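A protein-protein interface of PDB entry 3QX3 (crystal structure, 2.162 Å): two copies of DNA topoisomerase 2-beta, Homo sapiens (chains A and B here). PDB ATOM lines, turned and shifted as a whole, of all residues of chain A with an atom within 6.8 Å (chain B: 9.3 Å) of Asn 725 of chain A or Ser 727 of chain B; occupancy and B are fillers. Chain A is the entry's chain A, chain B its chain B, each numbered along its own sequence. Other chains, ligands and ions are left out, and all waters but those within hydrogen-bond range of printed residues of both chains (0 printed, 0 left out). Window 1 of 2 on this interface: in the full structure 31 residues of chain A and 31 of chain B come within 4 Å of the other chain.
Asn 725 of chain A touches two residues of chain B.
Of chain A, only Leu 724, Asn 725 and Met 726 come within 4 Å of Ser 727 of chain B.
Printed residues of chain B within 4 Å of Ile 663 of chain A: Leu 728 and Leu 731.
Of the printed residues of chain B, Met 726 of chain A touches Ser 727 (3.4 Å) and Leu 728 (3.0 Å).
Printed residues of chain B within 4 Å of Ile 723 of chain A: Leu 728 (3.7 Å).
Of the printed residues of chain B, Ser 727 of chain A touches Leu 724 (3.5 Å), Asn 725 (3.8 Å) and Met 726 (3.3 Å).
Of the printed residues of chain A, Leu 728 of chain B touches Ile 663, Ile 723, Leu 724, Met 726 and Leu 728.
The nearest residue of chain B that does not touch Asn 725 of chain A is Leu 728 of chain B (4.9 Å).
The backbone carbonyl oxygen of Leu 724 of chain A lies within hydrogen-bond range of the backbone NH of Leu 728 of chain B (3.2 Å).
NE1 of Trp 729 of chain B lies close to OD1 of Asn 725 of chain A.
The backbone NH (N) of Leu 728 of chain A lies within hydrogen-bond range of the backbone carbonyl oxygen (O) of Leu 724 of chain B (3.1 Å).
The backbone carbonyl oxygen (O) of Met 726 of chain B sits at hydrogen-bond distance from the backbone NH (N) of Leu 728 of chain A, at 2.9 Å.
The side-chain amide nitrogen (ND2) of Asn 721 of chain A sits close to the indole nitrogen (NE1) of Trp 729 of chain B.
O of Leu 724 of chain A is in hydrogen-bond range of N of Trp 729 of chain B.
The backbone carbonyl oxygen (O) of Met 726 of chain A sits at hydrogen-bond distance from the backbone NH (N) of Leu 728 of chain B (3.0 Å).
The backbone carbonyl oxygen (O) of Asn 721 of chain B sits close to the side-chain amide nitrogen (ND2) of Asn 725 of chain B, at 3.5 Å.
The backbone carbonyl oxygen of Ser 727 of chain B is in hydrogen-bond range of the side-chain hydroxyl of Ser 730 of chain B, 2.7 Å away.
O of Trp 729 of chain B sits at hydrogen-bond distance from OG1 of Thr 732 of chain B, at 2.7 Å.
OG of Ser 730 of chain A is in hydrogen-bond range of O of Ser 727 of chain A, at 2.8 Å.
The side-chain amide nitrogen (ND2) of Asn 725 of chain A lies close to the backbone carbonyl oxygen (O) of Asn 721 of chain A.
Among the printed residues, pairs that only touch across the chains: Ser 727 of chain A with Met 726 of chain B, Leu 728 of chain A with Ile 663 of chain B, Met 726 of chain A with Ser 727 of chain B, Ile 663 of chain A with Leu 728 of chain B, Ser 727 of chain A with Leu 724 of chain B, Leu 724 of chain A with Ser 727 of chain B, Leu 728 of chain A with Leu 728 of chain B, Leu 728 of chain A with Ile 723 of chain B, Ile 663 of chain A with Leu 731 of chain B, Ile 723 of chain A with Leu 728 of chain B, Asn 725 of chain A with Ser 727 of chain B, Leu 728 of chain A with Phe 652 of chain B, Ser 727 of chain A with Asn 725 of chain B and Leu 728 of chain A with Leu 731 of chain B.
Ile 663 of chain A touches Leu 728 of chain B, and with the chains exchanged Leu 728 of chain A touches Ile 663 of chain B.
Leu 724 of chain A touches Ser 727 of chain B, and with the chains exchanged Ser 727 of chain A touches Leu 724 of chain B.
Leu 724 of chain A touches Leu 728 of chain B, and with the chains exchanged Leu 728 of chain A touches Leu 724 of chain B.
Asn 725 of chain A touches Ser 727 of chain B, and with the chains exchanged Ser 727 of chain A touches Asn 725 of chain B.
Of the 21 pairs that touch across the chains among the printed residues, 15 have their exchanged pair printed and touching as well.
Of the 11 printed residues of chain A, 8 touch a printed residue of chain B.
Among the printed residues, 21 pairs touch across the chains.
Among the printed residues, no Asp or Glu carboxylate lies within 4 Å of a Lys or Arg side-chain nitrogen of the other chain.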
ATOM      1  N   ILE A 663     -25.014   8.826   8.351  1.00  0.00           N
ATOM      2  CA  ILE A 663     -24.077   8.053   9.139  1.00  0.00           C
ATOM      3  C   ILE A 663     -22.710   8.742   9.128  1.00  0.00           C
ATOM      4  O   ILE A 663     -21.825   8.417   9.923  1.00  0.00           O
ATOM      5  CB  ILE A 663     -23.980   6.619   8.601  1.00  0.00           C
ATOM      6  CG1 ILE A 663     -23.350   6.615   7.211  1.00  0.00           C
ATOM      7  CG2 ILE A 663     -25.369   5.993   8.523  1.00  0.00           C
ATOM      8  CD1 ILE A 663     -23.238   5.221   6.616  1.00  0.00           C
ATOM      9  N   PHE A 720     -26.110  -4.975  12.850  1.00  0.00           N
ATOM     10  CA  PHE A 720     -26.544  -4.195  11.696  1.00  0.00           C
ATOM     11  C   PHE A 720     -25.539  -4.249  10.547  1.00  0.00           C
ATOM     12  O   PHE A 720     -25.601  -3.452   9.602  1.00  0.00           O
ATOM     13  CB  PHE A 720     -26.850  -2.753  12.109  1.00  0.00           C
ATOM     14  CG  PHE A 720     -28.019  -2.631  13.054  1.00  0.00           C
ATOM     15  CD1 PHE A 720     -29.303  -2.965  12.636  1.00  0.00           C
ATOM     16  CD2 PHE A 720     -27.833  -2.192  14.360  1.00  0.00           C
ATOM     17  CE1 PHE A 720     -30.381  -2.860  13.494  1.00  0.00           C
ATOM     18  CE2 PHE A 720     -28.907  -2.086  15.231  1.00  0.00           C
ATOM     19  CZ  PHE A 720     -30.184  -2.417  14.799  1.00  0.00           C
ATOM     20  N   ASN A 721     -24.620  -5.208  10.627  1.00  0.00           N
ATOM     21  CA  ASN A 721     -23.651  -5.431   9.557  1.00  0.00           C
ATOM     22  C   ASN A 721     -24.262  -5.671   8.174  1.00  0.00           C
ATOM     23  O   ASN A 721     -23.705  -5.239   7.164  1.00  0.00           O
ATOM     24  CB  ASN A 721     -22.678  -6.556   9.930  1.00  0.00           C
ATOM     25  CG  ASN A 721     -21.657  -6.120  10.978  1.00  0.00           C
ATOM     26  OD1 ASN A 721     -21.579  -6.676  12.076  1.00  0.00           O
ATOM     27  ND2 ASN A 721     -20.875  -5.109  10.639  1.00  0.00           N
ATOM     28  N   TYR A 722     -25.406  -6.349   8.112  1.00  0.00           N
ATOM     29  CA  TYR A 722     -26.014  -6.642   6.809  1.00  0.00           C
ATOM     30  C   TYR A 722     -26.420  -5.364   6.073  1.00  0.00           C
ATOM     31  O   TYR A 722     -26.639  -5.366   4.855  1.00  0.00           O
ATOM     32  CB  TYR A 722     -27.219  -7.582   6.958  1.00  0.00           C
ATOM     33  CG  TYR A 722     -28.441  -6.975   7.618  1.00  0.00           C
ATOM     34  CD1 TYR A 722     -29.560  -6.650   6.871  1.00  0.00           C
ATOM     35  CD2 TYR A 722     -28.487  -6.766   8.990  1.00  0.00           C
ATOM     36  CE1 TYR A 722     -30.684  -6.119   7.464  1.00  0.00           C
ATOM     37  CE2 TYR A 722     -29.607  -6.223   9.590  1.00  0.00           C
ATOM     38  CZ  TYR A 722     -30.701  -5.910   8.823  1.00  0.00           C
ATOM     39  OH  TYR A 722     -31.824  -5.367   9.409  1.00  0.00           O
ATOM     40  N   ILE A 723     -26.551  -4.283   6.827  1.00  0.00           N
ATOM     41  CA  ILE A 723     -26.860  -2.981   6.246  1.00  0.00           C
ATOM     42  C   ILE A 723     -25.584  -2.194   5.930  1.00  0.00           C
ATOM     43  O   ILE A 723     -25.354  -1.784   4.795  1.00  0.00           O
ATOM     44  CB  ILE A 723     -27.720  -2.144   7.200  1.00  0.00           C
ATOM     45  CG1 ILE A 723     -29.069  -2.840   7.432  1.00  0.00           C
ATOM     46  CG2 ILE A 723     -27.917  -0.746   6.633  1.00  0.00           C
ATOM     47  CD1 ILE A 723     -29.943  -2.169   8.467  1.00  0.00           C
ATOM     48  N   LEU A 724     -24.751  -2.027   6.948  1.00  0.00           N
ATOM     49  CA  LEU A 724     -23.578  -1.176   6.868  1.00  0.00           C
ATOM     50  C   LEU A 724     -22.410  -1.780   6.081  1.00  0.00           C
ATOM     51  O   LEU A 724     -21.466  -1.072   5.752  1.00  0.00           O
ATOM     52  CB  LEU A 724     -23.145  -0.777   8.278  1.00  0.00           C
ATOM     53  CG  LEU A 724     -24.168   0.106   9.000  1.00  0.00           C
ATOM     54  CD1 LEU A 724     -23.795   0.292  10.459  1.00  0.00           C
ATOM     55  CD2 LEU A 724     -24.293   1.458   8.295  1.00  0.00           C
ATOM     56  N   ASN A 725     -22.480  -3.079   5.790  1.00  0.00           N
ATOM     57  CA  ASN A 725     -21.540  -3.748   4.873  1.00  0.00           C
ATOM     58  C   ASN A 725     -21.909  -3.549   3.409  1.00  0.00           C
ATOM     59  O   ASN A 725     -21.114  -3.835   2.521  1.00  0.00           O
ATOM     60  CB  ASN A 725     -21.458  -5.270   5.128  1.00  0.00           C
ATOM     61  CG  ASN A 725     -20.680  -5.617   6.381  1.00  0.00           C
ATOM     62  OD1 ASN A 725     -20.016  -4.767   6.964  1.00  0.00           O
ATOM     63  ND2 ASN A 725     -20.752  -6.884   6.795  1.00  0.00           N
ATOM     64  N   MET A 726     -23.118  -3.085   3.139  1.00  0.00           N
ATOM     65  CA  MET A 726     -23.466  -2.771   1.759  1.00  0.00           C
ATOM     66  C   MET A 726     -22.449  -1.757   1.220  1.00  0.00           C
ATOM     67  O   MET A 726     -21.984  -0.908   1.965  1.00  0.00           O
ATOM     68  CB  MET A 726     -24.886  -2.200   1.677  1.00  0.00           C
ATOM     69  CG  MET A 726     -25.991  -3.264   1.800  1.00  0.00           C
ATOM     70  SD  MET A 726     -27.648  -2.562   1.577  1.00  0.00           S
ATOM     71  CE  MET A 726     -27.780  -1.589   3.064  1.00  0.00           C
ATOM     72  N   SER A 727     -22.118  -1.842  -0.065  1.00  0.00           N
ATOM     73  CA  SER A 727     -21.154  -0.925  -0.669  1.00  0.00           C
ATOM     74  C   SER A 727     -21.762   0.460  -0.882  1.00  0.00           C
ATOM     75  O   SER A 727     -22.970   0.627  -0.802  1.00  0.00           O
ATOM     76  CB  SER A 727     -20.688  -1.460  -2.020  1.00  0.00           C
ATOM     77  OG  SER A 727     -21.762  -1.393  -2.944  1.00  0.00           O
ATOM     78  N   LEU A 728     -20.916   1.443  -1.176  1.00  0.00           N
ATOM     79  CA  LEU A 728     -21.370   2.798  -1.505  1.00  0.00           C
ATOM     80  C   LEU A 728     -22.164   2.823  -2.812  1.00  0.00           C
ATOM     81  O   LEU A 728     -23.047   3.661  -2.996  1.00  0.00           O
ATOM     82  CB  LEU A 728     -20.173   3.748  -1.583  1.00  0.00           C
ATOM     83  CG  LEU A 728     -19.492   3.970  -0.235  1.00  0.00           C
ATOM     84  CD1 LEU A 728     -18.125   4.636  -0.401  1.00  0.00           C
ATOM     85  CD2 LEU A 728     -20.400   4.809   0.655  1.00  0.00           C
ATOM     86  N   SER A 730     -24.467   1.047  -3.398  1.00  0.00           N
ATOM     87  CA  SER A 730     -25.854   0.874  -2.934  1.00  0.00           C
ATOM     88  C   SER A 730     -26.666   2.162  -2.999  1.00  0.00           C
ATOM     89  O   SER A 730     -27.867   2.126  -3.252  1.00  0.00           O
ATOM     90  CB  SER A 730     -25.888   0.361  -1.483  1.00  0.00           C
ATOM     91  OG  SER A 730     -25.267  -0.913  -1.355  1.00  0.00           O
ATOM     92  N   GLN B 649      -9.124   7.021  -2.064  1.00  0.00           N
ATOM     93  CA  GLN B 649     -10.170   6.537  -1.173  1.00  0.00           C
ATOM     94  C   GLN B 649     -10.384   7.504  -0.013  1.00  0.00           C
ATOM     95  O   GLN B 649     -11.519   7.847   0.300  1.00  0.00           O
ATOM     96  CB  GLN B 649      -9.835   5.141  -0.638  1.00  0.00           C
ATOM     97  CG  GLN B 649      -9.763   4.071  -1.699  1.00  0.00           C
ATOM     98  CD  GLN B 649      -9.347   2.716  -1.130  1.00  0.00           C
ATOM     99  OE1 GLN B 649      -9.956   1.688  -1.436  1.00  0.00           O
ATOM    100  NE2 GLN B 649      -8.321   2.716  -0.292  1.00  0.00           N
ATOM    101  N   PHE B 652     -12.004  10.808  -1.095  1.00  0.00           N
ATOM    102  CA  PHE B 652     -13.442  10.592  -1.297  1.00  0.00           C
ATOM    103  C   PHE B 652     -14.217  10.511   0.016  1.00  0.00           C
ATOM    104  O   PHE B 652     -15.279  11.109   0.151  1.00  0.00           O
ATOM    105  CB  PHE B 652     -13.731   9.344  -2.125  1.00  0.00           C
ATOM    106  CG  PHE B 652     -15.208   9.080  -2.304  1.00  0.00           C
ATOM    107  CD1 PHE B 652     -15.942   8.437  -1.312  1.00  0.00           C
ATOM    108  CD2 PHE B 652     -15.863   9.492  -3.458  1.00  0.00           C
ATOM    109  CE1 PHE B 652     -17.304   8.214  -1.473  1.00  0.00           C
ATOM    110  CE2 PHE B 652     -17.222   9.266  -3.631  1.00  0.00           C
ATOM    111  CZ  PHE B 652     -17.944   8.631  -2.637  1.00  0.00           C
ATOM    112  N   ILE B 653     -13.679   9.786   0.987  1.00  0.00           N
ATOM    113  CA  ILE B 653     -14.342   9.652   2.278  1.00  0.00           C
ATOM    114  C   ILE B 653     -14.421  11.005   3.013  1.00  0.00           C
ATOM    115  O   ILE B 653     -15.479  11.373   3.526  1.00  0.00           O
ATOM    116  CB  ILE B 653     -13.661   8.585   3.156  1.00  0.00           C
ATOM    117  CG1 ILE B 653     -13.864   7.181   2.561  1.00  0.00           C
ATOM    118  CG2 ILE B 653     -14.156   8.671   4.597  1.00  0.00           C
ATOM    119  CD1 ILE B 653     -15.319   6.678   2.605  1.00  0.00           C
ATOM    120  N   LYS B 656     -16.974  13.163   1.309  1.00  0.00           N
ATOM    121  CA  LYS B 656     -18.329  12.685   1.535  1.00  0.00           C
ATOM    122  C   LYS B 656     -18.830  13.133   2.896  1.00  0.00           C
ATOM    123  O   LYS B 656     -19.932  13.656   3.008  1.00  0.00           O
ATOM    124  CB  LYS B 656     -18.413  11.158   1.432  1.00  0.00           C
ATOM    125  CG  LYS B 656     -19.847  10.616   1.490  1.00  0.00           C
ATOM    126  CD  LYS B 656     -20.524  10.671   0.132  1.00  0.00           C
ATOM    127  CE  LYS B 656     -21.984  10.232   0.220  1.00  0.00           C
ATOM    128  NZ  LYS B 656     -22.775  10.989   1.238  1.00  0.00           N
ATOM    129  N   ILE B 663     -23.391  11.180  -3.567  1.00  0.00           N
ATOM    130  CA  ILE B 663     -23.593  10.177  -4.603  1.00  0.00           C
ATOM    131  C   ILE B 663     -25.026   9.659  -4.586  1.00  0.00           C
ATOM    132  O   ILE B 663     -25.457   8.979  -5.519  1.00  0.00           O
ATOM    133  CB  ILE B 663     -22.600   8.989  -4.452  1.00  0.00           C
ATOM    134  CG1 ILE B 663     -22.947   8.145  -3.232  1.00  0.00           C
ATOM    135  CG2 ILE B 663     -21.163   9.489  -4.336  1.00  0.00           C
ATOM    136  CD1 ILE B 663     -22.171   6.848  -3.165  1.00  0.00           C
ATOM    137  N   ASN B 721     -14.350   1.484  -8.978  1.00  0.00           N
ATOM    138  CA  ASN B 721     -14.832   0.420  -8.098  1.00  0.00           C
ATOM    139  C   ASN B 721     -14.128   0.371  -6.766  1.00  0.00           C
ATOM    140  O   ASN B 721     -14.749   0.094  -5.752  1.00  0.00           O
ATOM    141  CB  ASN B 721     -14.743  -0.948  -8.779  1.00  0.00           C
ATOM    142  CG  ASN B 721     -15.831  -1.146  -9.821  1.00  0.00           C
ATOM    143  OD1 ASN B 721     -15.598  -1.722 -10.880  1.00  0.00           O
ATOM    144  ND2 ASN B 721     -17.026  -0.649  -9.526  1.00  0.00           N
ATOM    145  N   TYR B 722     -12.830   0.659  -6.762  1.00  0.00           N
ATOM    146  CA  TYR B 722     -12.063   0.567  -5.529  1.00  0.00           C
ATOM    147  C   TYR B 722     -12.562   1.590  -4.519  1.00  0.00           C
ATOM    148  O   TYR B 722     -12.350   1.445  -3.316  1.00  0.00           O
ATOM    149  CB  TYR B 722     -10.564   0.756  -5.800  1.00  0.00           C
ATOM    150  CG  TYR B 722     -10.136   2.183  -6.143  1.00  0.00           C
ATOM    151  CD1 TYR B 722     -10.340   2.710  -7.415  1.00  0.00           C
ATOM    152  CD2 TYR B 722      -9.487   2.974  -5.204  1.00  0.00           C
ATOM    153  CE1 TYR B 722      -9.933   3.998  -7.734  1.00  0.00           C
ATOM    154  CE2 TYR B 722      -9.066   4.270  -5.514  1.00  0.00           C
ATOM    155  CZ  TYR B 722      -9.289   4.768  -6.780  1.00  0.00           C
ATOM    156  OH  TYR B 722      -8.882   6.043  -7.089  1.00  0.00           O
ATOM    157  N   ILE B 723     -13.210   2.636  -5.013  1.00  0.00           N
ATOM    158  CA  ILE B 723     -13.772   3.653  -4.129  1.00  0.00           C
ATOM    159  C   ILE B 723     -15.200   3.261  -3.743  1.00  0.00           C
ATOM    160  O   ILE B 723     -15.538   3.168  -2.566  1.00  0.00           O
ATOM    161  CB  ILE B 723     -13.786   5.039  -4.804  1.00  0.00           C
ATOM    162  CG1 ILE B 723     -12.357   5.531  -5.094  1.00  0.00           C
ATOM    163  CG2 ILE B 723     -14.504   6.042  -3.934  1.00  0.00           C
ATOM    164  CD1 ILE B 723     -12.339   6.817  -5.890  1.00  0.00           C
ATOM    165  N   LEU B 724     -16.023   2.996  -4.749  1.00  0.00           N
ATOM    166  CA  LEU B 724     -17.452   2.743  -4.525  1.00  0.00           C
ATOM    167  C   LEU B 724     -17.829   1.354  -3.974  1.00  0.00           C
ATOM    168  O   LEU B 724     -18.954   1.168  -3.505  1.00  0.00           O
ATOM    169  CB  LEU B 724     -18.236   3.034  -5.803  1.00  0.00           C
ATOM    170  CG  LEU B 724     -18.283   4.531  -6.101  1.00  0.00           C
ATOM    171  CD1 LEU B 724     -18.744   4.789  -7.518  1.00  0.00           C
ATOM    172  CD2 LEU B 724     -19.183   5.218  -5.088  1.00  0.00           C
ATOM    173  N   ASN B 725     -16.909   0.390  -4.047  1.00  0.00           N
ATOM    174  CA  ASN B 725     -17.072  -0.906  -3.369  1.00  0.00           C
ATOM    175  C   ASN B 725     -16.789  -0.847  -1.872  1.00  0.00           C
ATOM    176  O   ASN B 725     -16.976  -1.836  -1.170  1.00  0.00           O
ATOM    177  CB  ASN B 725     -16.163  -1.986  -3.959  1.00  0.00           C
ATOM    178  CG  ASN B 725     -16.596  -2.443  -5.333  1.00  0.00           C
ATOM    179  OD1 ASN B 725     -17.678  -2.116  -5.798  1.00  0.00           O
ATOM    180  ND2 ASN B 725     -15.740  -3.224  -5.990  1.00  0.00           N
ATOM    181  N   MET B 726     -16.301   0.283  -1.377  1.00  0.00           N
ATOM    182  CA  MET B 726     -16.105   0.423   0.063  1.00  0.00           C
ATOM    183  C   MET B 726     -17.476   0.358   0.736  1.00  0.00           C
ATOM    184  O   MET B 726     -18.482   0.772   0.155  1.00  0.00           O
ATOM    185  CB  MET B 726     -15.399   1.745   0.404  1.00  0.00           C
ATOM    186  CG  MET B 726     -13.924   1.826  -0.044  1.00  0.00           C
ATOM    187  SD  MET B 726     -13.225   3.476   0.278  1.00  0.00           S
ATOM    188  CE  MET B 726     -12.759   3.270   1.989  1.00  0.00           C
ATOM    189  N   SER B 727     -17.510  -0.166   1.954  1.00  0.00           N
ATOM    190  CA  SER B 727     -18.760  -0.328   2.680  1.00  0.00           C
ATOM    191  C   SER B 727     -19.193   0.988   3.301  1.00  0.00           C
ATOM    192  O   SER B 727     -18.378   1.888   3.498  1.00  0.00           O
ATOM    193  CB  SER B 727     -18.591  -1.358   3.787  1.00  0.00           C
ATOM    194  OG  SER B 727     -17.674  -0.887   4.757  1.00  0.00           O
ATOM    195  N   LEU B 728     -20.481   1.082   3.612  1.00  0.00           N
ATOM    196  CA  LEU B 728     -21.041   2.230   4.309  1.00  0.00           C
ATOM    197  C   LEU B 728     -20.357   2.484   5.643  1.00  0.00           C
ATOM    198  O   LEU B 728     -20.234   3.625   6.061  1.00  0.00           O
ATOM    199  CB  LEU B 728     -22.546   2.046   4.508  1.00  0.00           C
ATOM    200  CG  LEU B 728     -23.289   1.916   3.184  1.00  0.00           C
ATOM    201  CD1 LEU B 728     -24.769   1.606   3.412  1.00  0.00           C
ATOM    202  CD2 LEU B 728     -23.122   3.182   2.357  1.00  0.00           C
ATOM    203  N   TRP B 729     -19.920   1.421   6.311  1.00  0.00           N
ATOM    204  CA  TRP B 729     -19.090   1.550   7.505  1.00  0.00           C
ATOM    205  C   TRP B 729     -17.957   2.556   7.320  1.00  0.00           C
ATOM    206  O   TRP B 729     -17.524   3.196   8.273  1.00  0.00           O
ATOM    207  CB  TRP B 729     -18.443   0.207   7.843  1.00  0.00           C
ATOM    208  CG  TRP B 729     -19.279  -0.721   8.667  1.00  0.00           C
ATOM    209  CD1 TRP B 729     -19.623  -2.010   8.362  1.00  0.00           C
ATOM    210  CD2 TRP B 729     -19.859  -0.442   9.944  1.00  0.00           C
ATOM    211  NE1 TRP B 729     -20.390  -2.541   9.367  1.00  0.00           N
ATOM    212  CE2 TRP B 729     -20.546  -1.600  10.351  1.00  0.00           C
ATOM    213  CE3 TRP B 729     -19.865   0.681  10.783  1.00  0.00           C
ATOM    214  CZ2 TRP B 729     -21.232  -1.673  11.565  1.00  0.00           C
ATOM    215  CZ3 TRP B 729     -20.547   0.609  11.985  1.00  0.00           C
ATOM    216  CH2 TRP B 729     -21.223  -0.561  12.364  1.00  0.00           C
ATOM    217  N   SER B 730     -17.452   2.653   6.092  1.00  0.00           N
ATOM    218  CA  SER B 730     -16.320   3.516   5.763  1.00  0.00           C
ATOM    219  C   SER B 730     -16.595   4.979   6.090  1.00  0.00           C
ATOM    220  O   SER B 730     -15.667   5.751   6.256  1.00  0.00           O
ATOM    221  CB  SER B 730     -15.995   3.407   4.273  1.00  0.00           C
ATOM    222  OG  SER B 730     -15.681   2.067   3.938  1.00  0.00           O
ATOM    223  N   LEU B 731     -17.874   5.348   6.160  1.00  0.00           N
ATOM    224  CA  LEU B 731     -18.273   6.733   6.384  1.00  0.00           C
ATOM    225  C   LEU B 731     -18.317   7.088   7.861  1.00  0.00           C
ATOM    226  O   LEU B 731     -18.561   8.235   8.212  1.00  0.00           O
ATOM    227  CB  LEU B 731     -19.642   7.006   5.753  1.00  0.00           C
ATOM    228  CG  LEU B 731     -19.704   6.828   4.239  1.00  0.00           C
ATOM    229  CD1 LEU B 731     -21.128   7.074   3.722  1.00  0.00           C
ATOM    230  CD2 LEU B 731     -18.711   7.771   3.549  1.00  0.00           C
ATOM    231  N   THR B 732     -18.081   6.107   8.724  1.00  0.00           N
ATOM    232  CA  THR B 732     -18.239   6.317  10.160  1.00  0.00           C
ATOM    233  C   THR B 732     -16.912   6.701  10.796  1.00  0.00           C
ATOM    234  O   THR B 732     -15.848   6.456  10.227  1.00  0.00           O
ATOM    235  CB  THR B 732     -18.803   5.060  10.876  1.00  0.00           C
ATOM    236  OG1 THR B 732     -17.839   4.002  10.818  1.00  0.00           O
ATOM    237  CG2 THR B 732     -20.123   4.600  10.231  1.00  0.00           C
ATOM    238  N   LYS B 735     -13.755   4.395  11.247  1.00  0.00           N
ATOM    239  CA  LYS B 735     -13.237   3.915   9.974  1.00  0.00           C
ATOM    240  C   LYS B 735     -12.562   5.029   9.176  1.00  0.00           C
ATOM    241  O   LYS B 735     -11.679   4.766   8.359  1.00  0.00           O
ATOM    242  CB  LYS B 735     -14.350   3.285   9.132  1.00  0.00           C
ATOM    243  CG  LYS B 735     -15.071   2.125   9.796  1.00  0.00           C
ATOM    244  CD  LYS B 735     -14.143   0.971  10.137  1.00  0.00           C
ATOM    245  CE  LYS B 735     -13.660   0.247   8.898  1.00  0.00           C
ATOM    246  NZ  LYS B 735     -12.927  -1.007   9.270  1.00  0.00           N
ATOM    247  N   VAL B 736     -13.014   6.261   9.379  1.00  0.00           N
ATOM    248  CA  VAL B 736     -12.402   7.405   8.727  1.00  0.00           C
ATOM    249  C   VAL B 736     -10.997   7.589   9.275  1.00  0.00           C
ATOM    250  O   VAL B 736     -10.052   7.764   8.514  1.00  0.00           O
ATOM    251  CB  VAL B 736     -13.183   8.693   8.975  1.00  0.00           C
ATOM    252  CG1 VAL B 736     -12.392   9.881   8.469  1.00  0.00           C
ATOM    253  CG2 VAL B 736     -14.548   8.629   8.306  1.00  0.00           C
ATOM    254  N   LEU B 739      -8.757   4.756   8.099  1.00  0.00           N
ATOM    255  CA  LEU B 739      -8.349   4.963   6.720  1.00  0.00           C
ATOM    256  C   LEU B 739      -7.235   6.025   6.595  1.00  0.00           C
ATOM    257  O   LEU B 739      -6.316   5.877   5.792  1.00  0.00           O
ATOM    258  CB  LEU B 739      -9.556   5.354   5.874  1.00  0.00           C
ATOM    259  CG  LEU B 739      -9.298   5.675   4.408  1.00  0.00           C
ATOM    260  CD1 LEU B 739      -8.609   4.502   3.751  1.00  0.00           C
ATOM    261  CD2 LEU B 739     -10.604   5.971   3.733  1.00  0.00           C
